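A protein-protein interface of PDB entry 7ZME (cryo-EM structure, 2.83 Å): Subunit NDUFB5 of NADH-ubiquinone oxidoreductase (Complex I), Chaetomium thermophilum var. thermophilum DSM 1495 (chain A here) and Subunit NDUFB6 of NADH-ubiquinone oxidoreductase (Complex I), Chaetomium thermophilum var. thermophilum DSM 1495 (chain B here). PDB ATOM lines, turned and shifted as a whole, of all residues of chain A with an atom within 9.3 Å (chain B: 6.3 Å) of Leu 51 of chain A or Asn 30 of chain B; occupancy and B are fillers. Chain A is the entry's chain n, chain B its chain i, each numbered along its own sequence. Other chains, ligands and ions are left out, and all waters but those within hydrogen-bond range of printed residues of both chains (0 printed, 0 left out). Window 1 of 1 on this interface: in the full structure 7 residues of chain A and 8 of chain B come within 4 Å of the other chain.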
ATOM      1  N   VAL A  47      35.405  -4.050  -5.060  1.00  0.00           N
ATOM      2  CA  VAL A  47      34.040  -4.430  -5.531  1.00  0.00           C
ATOM      3  C   VAL A  47      33.085  -4.489  -4.335  1.00  0.00           C
ATOM      4  O   VAL A  47      33.510  -4.973  -3.271  1.00  0.00           O
ATOM      5  CB  VAL A  47      34.078  -5.772  -6.283  1.00  0.00           C
ATOM      6  CG1 VAL A  47      32.783  -6.038  -7.035  1.00  0.00           C
ATOM      7  CG2 VAL A  47      35.268  -5.850  -7.227  1.00  0.00           C
ATOM      8  N   GLU A  48      31.847  -4.018  -4.501  1.00  0.00           N
ATOM      9  CA  GLU A  48      30.828  -4.075  -3.417  1.00  0.00           C
ATOM     10  C   GLU A  48      30.211  -5.477  -3.373  1.00  0.00           C
ATOM     11  O   GLU A  48      30.272  -6.167  -4.405  1.00  0.00           O
ATOM     12  CB  GLU A  48      29.733  -3.052  -3.710  1.00  0.00           C
ATOM     13  CG  GLU A  48      28.972  -2.603  -2.481  1.00  0.00           C
ATOM     14  CD  GLU A  48      27.662  -1.891  -2.763  1.00  0.00           C
ATOM     15  OE1 GLU A  48      27.386  -1.608  -3.945  1.00  0.00           O
ATOM     16  OE2 GLU A  48      26.918  -1.625  -1.798  1.00  0.00           O
ATOM     17  N   GLU A  49      29.626  -5.866  -2.229  1.00  0.00           N
ATOM     18  CA  GLU A  49      28.941  -7.184  -2.108  1.00  0.00           C
ATOM     19  C   GLU A  49      27.424  -7.001  -1.949  1.00  0.00           C
ATOM     20  O   GLU A  49      27.031  -6.313  -0.998  1.00  0.00           O
ATOM     21  CB  GLU A  49      29.455  -7.999  -0.922  1.00  0.00           C
ATOM     22  CG  GLU A  49      30.448  -9.075  -1.316  1.00  0.00           C
ATOM     23  CD  GLU A  49      29.845 -10.229  -2.096  1.00  0.00           C
ATOM     24  OE1 GLU A  49      28.736 -10.664  -1.740  1.00  0.00           O
ATOM     25  OE2 GLU A  49      30.486 -10.686  -3.063  1.00  0.00           O
ATOM     26  N   PRO A  50      26.534  -7.593  -2.789  1.00  0.00           N
ATOM     27  CA  PRO A  50      25.100  -7.486  -2.532  1.00  0.00           C
ATOM     28  C   PRO A  50      24.762  -8.342  -1.303  1.00  0.00           C
ATOM     29  O   PRO A  50      25.449  -9.314  -1.072  1.00  0.00           O
ATOM     30  CB  PRO A  50      24.476  -8.093  -3.795  1.00  0.00           C
ATOM     31  CG  PRO A  50      25.533  -9.034  -4.332  1.00  0.00           C
ATOM     32  CD  PRO A  50      26.860  -8.402  -3.962  1.00  0.00           C
ATOM     33  N   LEU A  51      23.698  -8.002  -0.570  1.00  0.00           N
ATOM     34  CA  LEU A  51      23.307  -8.885   0.555  1.00  0.00           C
ATOM     35  C   LEU A  51      22.996 -10.243  -0.048  1.00  0.00           C
ATOM     36  O   LEU A  51      23.472 -11.251   0.507  1.00  0.00           O
ATOM     37  CB  LEU A  51      22.071  -8.330   1.258  1.00  0.00           C
ATOM     38  CG  LEU A  51      22.326  -7.206   2.254  1.00  0.00           C
ATOM     39  CD1 LEU A  51      21.019  -6.774   2.895  1.00  0.00           C
ATOM     40  CD2 LEU A  51      23.324  -7.642   3.315  1.00  0.00           C
ATOM     41  N   GLY A  52      22.261 -10.271  -1.154  1.00  0.00           N
ATOM     42  CA  GLY A  52      22.066 -11.569  -1.824  1.00  0.00           C
ATOM     43  C   GLY A  52      20.751 -12.238  -1.503  1.00  0.00           C
ATOM     44  O   GLY A  52      20.259 -12.053  -0.390  1.00  0.00           O
ATOM     45  N   ALA A  53      20.227 -13.029  -2.441  1.00  0.00           N
ATOM     46  CA  ALA A  53      18.911 -13.625  -2.246  1.00  0.00           C
ATOM     47  C   ALA A  53      18.870 -14.521  -1.016  1.00  0.00           C
ATOM     48  O   ALA A  53      17.837 -14.596  -0.342  1.00  0.00           O
ATOM     49  CB  ALA A  53      18.501 -14.413  -3.488  1.00  0.00           C
ATOM     50  N   ALA A  54      19.977 -15.204  -0.708  1.00  0.00           N
ATOM     51  CA  ALA A  54      20.005 -16.093   0.449  1.00  0.00           C
ATOM     52  C   ALA A  54      19.724 -15.335   1.738  1.00  0.00           C
ATOM     53  O   ALA A  54      19.133 -15.885   2.674  1.00  0.00           O
ATOM     54  CB  ALA A  54      21.351 -16.808   0.532  1.00  0.00           C
ATOM     55  N   PHE A  55      20.149 -14.072   1.809  1.00  0.00           N
ATOM     56  CA  PHE A  55      19.850 -13.258   2.983  1.00  0.00           C
ATOM     57  C   PHE A  55      18.347 -13.098   3.165  1.00  0.00           C
ATOM     58  O   PHE A  55      17.823 -13.249   4.273  1.00  0.00           O
ATOM     59  CB  PHE A  55      20.526 -11.892   2.861  1.00  0.00           C
ATOM     60  CG  PHE A  55      20.152 -10.931   3.954  1.00  0.00           C
ATOM     61  CD1 PHE A  55      20.839 -10.930   5.154  1.00  0.00           C
ATOM     62  CD2 PHE A  55      19.120 -10.024   3.779  1.00  0.00           C
ATOM     63  CE1 PHE A  55      20.504 -10.052   6.161  1.00  0.00           C
ATOM     64  CE2 PHE A  55      18.777  -9.144   4.783  1.00  0.00           C
ATOM     65  CZ  PHE A  55      19.470  -9.157   5.977  1.00  0.00           C
ATOM     66  N   TYR A  56      17.636 -12.800   2.077  1.00  0.00           N
ATOM     67  CA  TYR A  56      16.197 -12.581   2.173  1.00  0.00           C
ATOM     68  C   TYR A  56      15.434 -13.890   2.319  1.00  0.00           C
ATOM     69  O   TYR A  56      14.381 -13.921   2.962  1.00  0.00           O
ATOM     70  CB  TYR A  56      15.710 -11.802   0.952  1.00  0.00           C
ATOM     71  CG  TYR A  56      16.466 -10.513   0.730  1.00  0.00           C
ATOM     72  CD1 TYR A  56      16.372  -9.467   1.637  1.00  0.00           C
ATOM     73  CD2 TYR A  56      17.283 -10.347  -0.379  1.00  0.00           C
ATOM     74  CE1 TYR A  56      17.063  -8.288   1.442  1.00  0.00           C
ATOM     75  CE2 TYR A  56      17.979  -9.172  -0.583  1.00  0.00           C
ATOM     76  CZ  TYR A  56      17.865  -8.146   0.331  1.00  0.00           C
ATOM     77  OH  TYR A  56      18.557  -6.973   0.133  1.00  0.00           O
ATOM     78  N   ILE A  57      15.936 -14.973   1.724  1.00  0.00           N
ATOM     79  CA  ILE A  57      15.284 -16.267   1.888  1.00  0.00           C
ATOM     80  C   ILE A  57      15.358 -16.720   3.340  1.00  0.00           C
ATOM     81  O   ILE A  57      14.375 -17.218   3.901  1.00  0.00           O
ATOM     82  CB  ILE A  57      15.908 -17.301   0.934  1.00  0.00           C
ATOM     83  CG1 ILE A  57      15.633 -16.907  -0.517  1.00  0.00           C
ATOM     84  CG2 ILE A  57      15.360 -18.687   1.215  1.00  0.00           C
ATOM     85  CD1 ILE A  57      16.530 -17.594  -1.515  1.00  0.00           C
ATOM     86  N   VAL A  59      16.052 -14.627   6.048  1.00  0.00           N
ATOM     87  CA  VAL A  59      15.345 -13.637   6.855  1.00  0.00           C
ATOM     88  C   VAL A  59      13.846 -13.713   6.603  1.00  0.00           C
ATOM     89  O   VAL A  59      13.042 -13.693   7.542  1.00  0.00           O
ATOM     90  CB  VAL A  59      15.899 -12.227   6.582  1.00  0.00           C
ATOM     91  CG1 VAL A  59      14.906 -11.166   7.029  1.00  0.00           C
ATOM     92  CG2 VAL A  59      17.235 -12.038   7.281  1.00  0.00           C
ATOM     93  N   PRO B  24      34.547  -7.208   1.998  1.00  0.00           N
ATOM     94  CA  PRO B  24      33.835  -6.440   1.018  1.00  0.00           C
ATOM     95  C   PRO B  24      34.072  -4.934   1.216  1.00  0.00           C
ATOM     96  O   PRO B  24      34.553  -4.538   2.254  1.00  0.00           O
ATOM     97  CB  PRO B  24      32.403  -6.929   1.241  1.00  0.00           C
ATOM     98  CG  PRO B  24      32.342  -7.208   2.692  1.00  0.00           C
ATOM     99  CD  PRO B  24      33.676  -7.858   2.954  1.00  0.00           C
ATOM    100  N   ASN B  26      31.731  -2.865   1.294  1.00  0.00           N
ATOM    101  CA  ASN B  26      30.559  -2.402   2.063  1.00  0.00           C
ATOM    102  C   ASN B  26      30.482  -3.149   3.382  1.00  0.00           C
ATOM    103  O   ASN B  26      29.413  -3.158   3.953  1.00  0.00           O
ATOM    104  CB  ASN B  26      29.268  -2.532   1.261  1.00  0.00           C
ATOM    105  CG  ASN B  26      29.053  -3.883   0.622  1.00  0.00           C
ATOM    106  OD1 ASN B  26      29.997  -4.554   0.224  1.00  0.00           O
ATOM    107  ND2 ASN B  26      27.797  -4.264   0.479  1.00  0.00           N
ATOM    108  N   TRP B  27      31.588  -3.668   3.887  1.00  0.00           N
ATOM    109  CA  TRP B  27      31.554  -4.525   5.097  1.00  0.00           C
ATOM    110  C   TRP B  27      30.758  -3.887   6.240  1.00  0.00           C
ATOM    111  O   TRP B  27      29.926  -4.566   6.815  1.00  0.00           O
ATOM    112  CB  TRP B  27      32.955  -4.996   5.485  1.00  0.00           C
ATOM    113  CG  TRP B  27      33.803  -4.034   6.257  1.00  0.00           C
ATOM    114  CD1 TRP B  27      34.779  -3.230   5.756  1.00  0.00           C
ATOM    115  CD2 TRP B  27      33.796  -3.816   7.680  1.00  0.00           C
ATOM    116  NE1 TRP B  27      35.362  -2.511   6.759  1.00  0.00           N
ATOM    117  CE2 TRP B  27      34.778  -2.847   7.949  1.00  0.00           C
ATOM    118  CE3 TRP B  27      33.042  -4.315   8.743  1.00  0.00           C
ATOM    119  CZ2 TRP B  27      35.030  -2.378   9.236  1.00  0.00           C
ATOM    120  CZ3 TRP B  27      33.287  -3.851  10.014  1.00  0.00           C
ATOM    121  CH2 TRP B  27      34.269  -2.896  10.256  1.00  0.00           C
ATOM    122  N   LYS B  28      30.994  -2.612   6.512  1.00  0.00           N
ATOM    123  CA  LYS B  28      30.304  -1.893   7.578  1.00  0.00           C
ATOM    124  C   LYS B  28      28.811  -1.810   7.308  1.00  0.00           C
ATOM    125  O   LYS B  28      27.995  -1.937   8.228  1.00  0.00           O
ATOM    126  CB  LYS B  28      30.891  -0.493   7.735  1.00  0.00           C
ATOM    127  CG  LYS B  28      32.313  -0.458   8.246  1.00  0.00           C
ATOM    128  CD  LYS B  28      32.769   0.971   8.491  1.00  0.00           C
ATOM    129  CE  LYS B  28      34.272   1.049   8.683  1.00  0.00           C
ATOM    130  NZ  LYS B  28      35.006   0.652   7.452  1.00  0.00           N
ATOM    131  N   GLN B  29      28.387  -1.614   6.070  1.00  0.00           N
ATOM    132  CA  GLN B  29      26.958  -1.372   5.781  1.00  0.00           C
ATOM    133  C   GLN B  29      26.207  -2.665   5.976  1.00  0.00           C
ATOM    134  O   GLN B  29      25.083  -2.616   6.485  1.00  0.00           O
ATOM    135  CB  GLN B  29      26.835  -0.874   4.344  1.00  0.00           C
ATOM    136  CG  GLN B  29      25.436  -0.416   3.963  1.00  0.00           C
ATOM    137  CD  GLN B  29      25.212  -0.538   2.476  1.00  0.00           C
ATOM    138  OE1 GLN B  29      24.281   0.037   1.918  1.00  0.00           O
ATOM    139  NE2 GLN B  29      26.077  -1.295   1.823  1.00  0.00           N
ATOM    140  N   ASN B  30      26.857  -3.766   5.635  1.00  0.00           N
ATOM    141  CA  ASN B  30      26.214  -5.095   5.717  1.00  0.00           C
ATOM    142  C   ASN B  30      26.327  -5.619   7.145  1.00  0.00           C
ATOM    143  O   ASN B  30      25.447  -6.392   7.552  1.00  0.00           O
ATOM    144  CB  ASN B  30      26.760  -5.960   4.589  1.00  0.00           C
ATOM    145  CG  ASN B  30      26.519  -5.251   3.275  1.00  0.00           C
ATOM    146  OD1 ASN B  30      27.097  -4.203   3.023  1.00  0.00           O
ATOM    147  ND2 ASN B  30      25.610  -5.760   2.465  1.00  0.00           N
ATOM    148  N   THR B  31      27.356  -5.177   7.869  1.00  0.00           N
ATOM    149  CA  THR B  31      27.529  -5.642   9.262  1.00  0.00           C
ATOM    150  C   THR B  31      26.423  -4.979  10.054  1.00  0.00           C
ATOM    151  O   THR B  31      25.855  -5.641  10.939  1.00  0.00           O
ATOM    152  CB  THR B  31      28.980  -5.530   9.739  1.00  0.00           C
ATOM    153  OG1 THR B  31      29.777  -6.390   8.931  1.00  0.00           O
ATOM    154  CG2 THR B  31      29.174  -5.887  11.195  1.00  0.00           C
ATOM    155  N   ALA B  32      26.104  -3.737   9.708  1.00  0.00           N
ATOM    156  CA  ALA B  32      24.983  -3.042  10.329  1.00  0.00           C
ATOM    157  C   ALA B  32      23.674  -3.769  10.059  1.00  0.00           C
ATOM    158  O   ALA B  32      22.852  -3.940  10.965  1.00  0.00           O
ATOM    159  CB  ALA B  32      24.916  -1.603   9.821  1.00  0.00           C
ATOM    160  N   ILE B  33      23.468  -4.214   8.818  1.00  0.00           N
ATOM    161  CA  ILE B  33      22.231  -4.902   8.463  1.00  0.00           C
ATOM    162  C   ILE B  33      22.115  -6.217   9.222  1.00  0.00           C
ATOM    163  O   ILE B  33      21.057  -6.549   9.768  1.00  0.00           O
ATOM    164  CB  ILE B  33      22.160  -5.120   6.942  1.00  0.00           C
ATOM    165  CG1 ILE B  33      22.027  -3.783   6.220  1.00  0.00           C
ATOM    166  CG2 ILE B  33      21.001  -6.029   6.585  1.00  0.00           C
ATOM    167  CD1 ILE B  33      22.047  -3.907   4.717  1.00  0.00           C
ATOM    168  N   PHE B  34      23.201  -6.990   9.267  1.00  0.00           N
ATOM    169  CA  PHE B  34      23.163  -8.265   9.973  1.00  0.00           C
ATOM    170  C   PHE B  34      23.048  -8.076  11.478  1.00  0.00           C
ATOM    171  O   PHE B  34      22.382  -8.871  12.149  1.00  0.00           O
ATOM    172  CB  PHE B  34      24.401  -9.092   9.635  1.00  0.00           C
ATOM    173  CG  PHE B  34      24.232  -9.962   8.432  1.00  0.00           C
ATOM    174  CD1 PHE B  34      23.482 -11.116   8.501  1.00  0.00           C
ATOM    175  CD2 PHE B  34      24.812  -9.619   7.227  1.00  0.00           C
ATOM    176  CE1 PHE B  34      23.324 -11.917   7.397  1.00  0.00           C
ATOM    177  CE2 PHE B  34      24.655 -10.415   6.119  1.00  0.00           C
ATOM    178  CZ  PHE B  34      23.911 -11.565   6.206  1.00  0.00           C
ATOM    179  N   GLY B  35      23.690  -7.043  12.025  1.00  0.00           N
ATOM    180  CA  GLY B  35      23.562  -6.771  13.445  1.00  0.00           C
ATOM    181  C   GLY B  35      22.148  -6.420  13.854  1.00  0.00           C
ATOM    182  O   GLY B  35      21.722  -6.742  14.966  1.00  0.00           O
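Leu 51 of chain A touches just these residues of chain B: Asn 30 (3.1 Å) and Ile 33 (3.5 Å). Asn 30 of chain B touches two residues of chain A. Of the printed residues of chain A, Asn 26 of chain B touches Glu 48 (3.4 Å) and Glu 49 (2.6 Å). No residue of chain A comes within 4 Å of Ala 32 of chain B. Of the printed residues of chain A, Ile 33 of chain B touches Leu 51 (3.5 Å) and Phe 55 (3.5 Å). Of the printed residues of chain B, Glu 49 of chain A touches Pro 24 (3.8 Å), Asn 26 (2.6 Å) and Asn 30 (3.8 Å). Printed residues of chain B within 4 Å of Phe 55 of chain A: Ile 33 and Phe 34. Ile 57 of chain A touches none of the printed residues of chain B. Val 47 of chain A touches none of the printed residues of chain B. The nearest residue of chain B that does not touch Leu 51 of chain A is Phe 34 of chain B (4.2 Å). The nearest residue of chain A that does not touch Asn 30 of chain B is Pro 50 of chain A (4.6 Å). The nearest printed residue of chain B that does not touch Phe 55 of chain A is Asn 30 of chain B (6.3 Å).
The side-chain amide oxygen of Asn 30 of chain B sits at hydrogen-bond distance from the side-chain amide nitrogen of Asn 26 of chain B. The side-chain amide nitrogen of Gln 29 of chain B is in hydrogen-bond range of the side-chain amide oxygen of Asn 30 of chain B, at 3.3 Å.
The backbone carbonyl oxygen (O) of Glu 49 of chain A lies within hydrogen-bond range of the side-chain amide nitrogen (ND2) of Asn 26 of chain B, at 2.6 Å.
Of the 12 printed residues of chain A, 4 touch a printed residue of chain B. Of the 11 printed residues of chain B, 6 touch a printed residue of chain A. Hydrophobic or aromatic side chains of chain B within 4 Å of the printed part of chain A: Pro 24, Ile 33 and Phe 34.
CG of Glu 48 of chain A touches CG of Asn 26 of chain B (3.4 Å). Gln 29 of chain B touches Glu 48 of chain A. Glu 49 of chain A touches Pro 24 of chain B (CB to CB, 3.8 Å). ND2 of Asn 30 of chain B touches O of Glu 49 of chain A (3.8 Å). Asn 30 of chain B touches Leu 51 of chain A. Leu 51 of chain A touches Ile 33 of chain B. Ile 33 of chain B touches Phe 55 of chain A (CG2 to CZ, 3.5 Å). Phe 55 of chain A touches Phe 34 of chain B (CD1 to CZ, 3.3 Å).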
